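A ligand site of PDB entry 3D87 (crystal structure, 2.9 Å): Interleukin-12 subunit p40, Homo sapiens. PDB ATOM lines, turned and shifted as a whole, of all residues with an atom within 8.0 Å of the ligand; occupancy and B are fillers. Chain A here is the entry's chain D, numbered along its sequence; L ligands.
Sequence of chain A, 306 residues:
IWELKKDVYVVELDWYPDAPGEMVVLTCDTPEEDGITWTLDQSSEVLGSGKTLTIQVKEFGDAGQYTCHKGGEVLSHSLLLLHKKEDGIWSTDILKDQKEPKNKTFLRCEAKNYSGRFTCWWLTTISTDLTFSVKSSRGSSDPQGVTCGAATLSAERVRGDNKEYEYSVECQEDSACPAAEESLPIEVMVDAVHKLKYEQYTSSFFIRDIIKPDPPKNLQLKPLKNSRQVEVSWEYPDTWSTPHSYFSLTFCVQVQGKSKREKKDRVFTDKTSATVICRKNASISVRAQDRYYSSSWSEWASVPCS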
ATOM      1  N   VAL A 255      12.711 -10.124  -8.781  1.00  0.00           N
ATOM      2  CA  VAL A 255      13.726  -9.860  -7.753  1.00  0.00           C
ATOM      3  C   VAL A 255      14.668 -11.038  -7.476  1.00  0.00           C
ATOM      4  O   VAL A 255      14.342 -11.961  -6.741  1.00  0.00           O
ATOM      5  CB  VAL A 255      13.073  -9.281  -6.474  1.00  0.00           C
ATOM      6  CG1 VAL A 255      12.843  -7.758  -6.608  1.00  0.00           C
ATOM      7  CG2 VAL A 255      11.754  -9.995  -6.163  1.00  0.00           C
ATOM      8  N   ASP A 265       7.836 -10.353  -4.575  1.00  0.00           N
ATOM      9  CA  ASP A 265       6.839 -10.477  -5.644  1.00  0.00           C
ATOM     10  C   ASP A 265       7.112  -9.523  -6.816  1.00  0.00           C
ATOM     11  O   ASP A 265       7.774  -8.494  -6.662  1.00  0.00           O
ATOM     12  CB  ASP A 265       5.400 -10.317  -5.106  1.00  0.00           C
ATOM     13  CG  ASP A 265       4.412 -11.278  -5.779  1.00  0.00           C
ATOM     14  OD1 ASP A 265       4.822 -12.364  -6.234  1.00  0.00           O
ATOM     15  OD2 ASP A 265       3.212 -10.934  -5.873  1.00  0.00           O
ATOM     16  N   ARG A 279      18.067  -6.245  -2.184  1.00  0.00           N
ATOM     17  CA  ARG A 279      19.008  -6.855  -1.257  1.00  0.00           C
ATOM     18  C   ARG A 279      20.077  -7.586  -2.072  1.00  0.00           C
ATOM     19  O   ARG A 279      19.856  -7.909  -3.236  1.00  0.00           O
ATOM     20  CB  ARG A 279      18.280  -7.825  -0.321  1.00  0.00           C
ATOM     21  CG  ARG A 279      17.043  -7.216   0.356  1.00  0.00           C
ATOM     22  CD  ARG A 279      15.794  -7.961  -0.055  1.00  0.00           C
ATOM     23  NE  ARG A 279      16.105  -9.326  -0.463  1.00  0.00           N
ATOM     24  CZ  ARG A 279      15.256 -10.133  -1.080  1.00  0.00           C
ATOM     25  NH1 ARG A 279      14.026  -9.700  -1.377  1.00  0.00           N
ATOM     26  NH2 ARG A 279      15.627 -11.370  -1.408  1.00  0.00           N
ATOM     27  N   LYS A 280      21.242  -7.818  -1.488  1.00  0.00           N
ATOM     28  CA  LYS A 280      22.313  -8.465  -2.226  1.00  0.00           C
ATOM     29  C   LYS A 280      21.951  -9.904  -2.614  1.00  0.00           C
ATOM     30  O   LYS A 280      22.596 -10.494  -3.476  1.00  0.00           O
ATOM     31  CB  LYS A 280      23.635  -8.410  -1.448  1.00  0.00           C
ATOM     32  CG  LYS A 280      23.780  -7.165  -0.580  1.00  0.00           C
ATOM     33  N   ASN A 281      20.906 -10.441  -1.982  1.00  0.00           N
ATOM     34  CA  ASN A 281      20.405 -11.805  -2.251  1.00  0.00           C
ATOM     35  C   ASN A 281      20.362 -12.130  -3.762  1.00  0.00           C
ATOM     36  O   ASN A 281      21.396 -12.476  -4.368  1.00  0.00           O
ATOM     37  CB  ASN A 281      19.002 -11.990  -1.632  1.00  0.00           C
ATOM     38  CG  ASN A 281      18.822 -13.361  -0.965  1.00  0.00           C
ATOM     39  OD1 ASN A 281      18.243 -13.460   0.117  1.00  0.00           O
ATOM     40  ND2 ASN A 281      19.241 -14.428  -1.654  1.00  0.00           N
ATOM     41  N   ALA A 282      19.164 -12.025  -4.353  1.00  0.00           N
ATOM     42  CA  ALA A 282      18.957 -12.300  -5.782  1.00  0.00           C
ATOM     43  C   ALA A 282      19.531 -11.187  -6.663  1.00  0.00           C
ATOM     44  O   ALA A 282      20.674 -10.746  -6.485  1.00  0.00           O
ATOM     45  CB  ALA A 282      17.463 -12.505  -6.101  1.00  0.00           C
ATOM     46  N   SER A 283      18.742 -10.783  -7.655  1.00  0.00           N
ATOM     47  CA  SER A 283      19.124  -9.736  -8.597  1.00  0.00           C
ATOM     48  C   SER A 283      17.829  -9.250  -9.234  1.00  0.00           C
ATOM     49  O   SER A 283      16.761  -9.835  -9.000  1.00  0.00           O
ATOM     50  CB  SER A 283      20.060 -10.290  -9.686  1.00  0.00           C
ATOM     51  OG  SER A 283      21.244 -10.852  -9.136  1.00  0.00           O
HETATM   52  C1  LIG L   1      16.167 -14.442  -4.283  1.00  0.00           C
HETATM   53  C2  LIG L   1      16.928 -15.804  -4.370  1.00  0.00           C
HETATM   54  C3  LIG L   1      15.995 -17.033  -4.049  1.00  0.00           C
HETATM   55  C4  LIG L   1      14.756 -16.752  -3.076  1.00  0.00           C
HETATM   56  C5  LIG L   1      14.263 -15.259  -3.051  1.00  0.00           C
HETATM   57  C6  LIG L   1      13.203 -14.954  -1.932  1.00  0.00           C
HETATM   58  O1  LIG L   1      18.210 -15.816  -3.660  1.00  0.00           O
HETATM   59  O2  LIG L   1      16.755 -18.200  -3.670  1.00  0.00           O
HETATM   60  O3  LIG L   1      13.665 -17.686  -3.299  1.00  0.00           O
HETATM   61  O4  LIG L   1      15.369 -14.310  -3.084  1.00  0.00           O
HETATM   62  O5  LIG L   1      13.024 -13.531  -1.616  1.00  0.00           O
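An oxygen (O1) of the ligand is in hydrogen-bond range of the side-chain amide nitrogen (ND2) of Asn 281 (2.6 Å).
An oxygen (O5) of the ligand lies within hydrogen-bond range of the guanidinium group (NH2) of Arg 279, at 3.4 Å.
O of Val 255 touches C1 of the ligand, 3.9 Å away.
Ala 282 touches the ligand (CB to C1, 3.0 Å).
Hydrophobic or aromatic side chains that line the ligand: Ala 282.
Of the 7 residues printed, 4 come within 4 Å of the ligand.
The nearest printed residue that does not touch the ligand is Ser 283 (5.6 Å).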
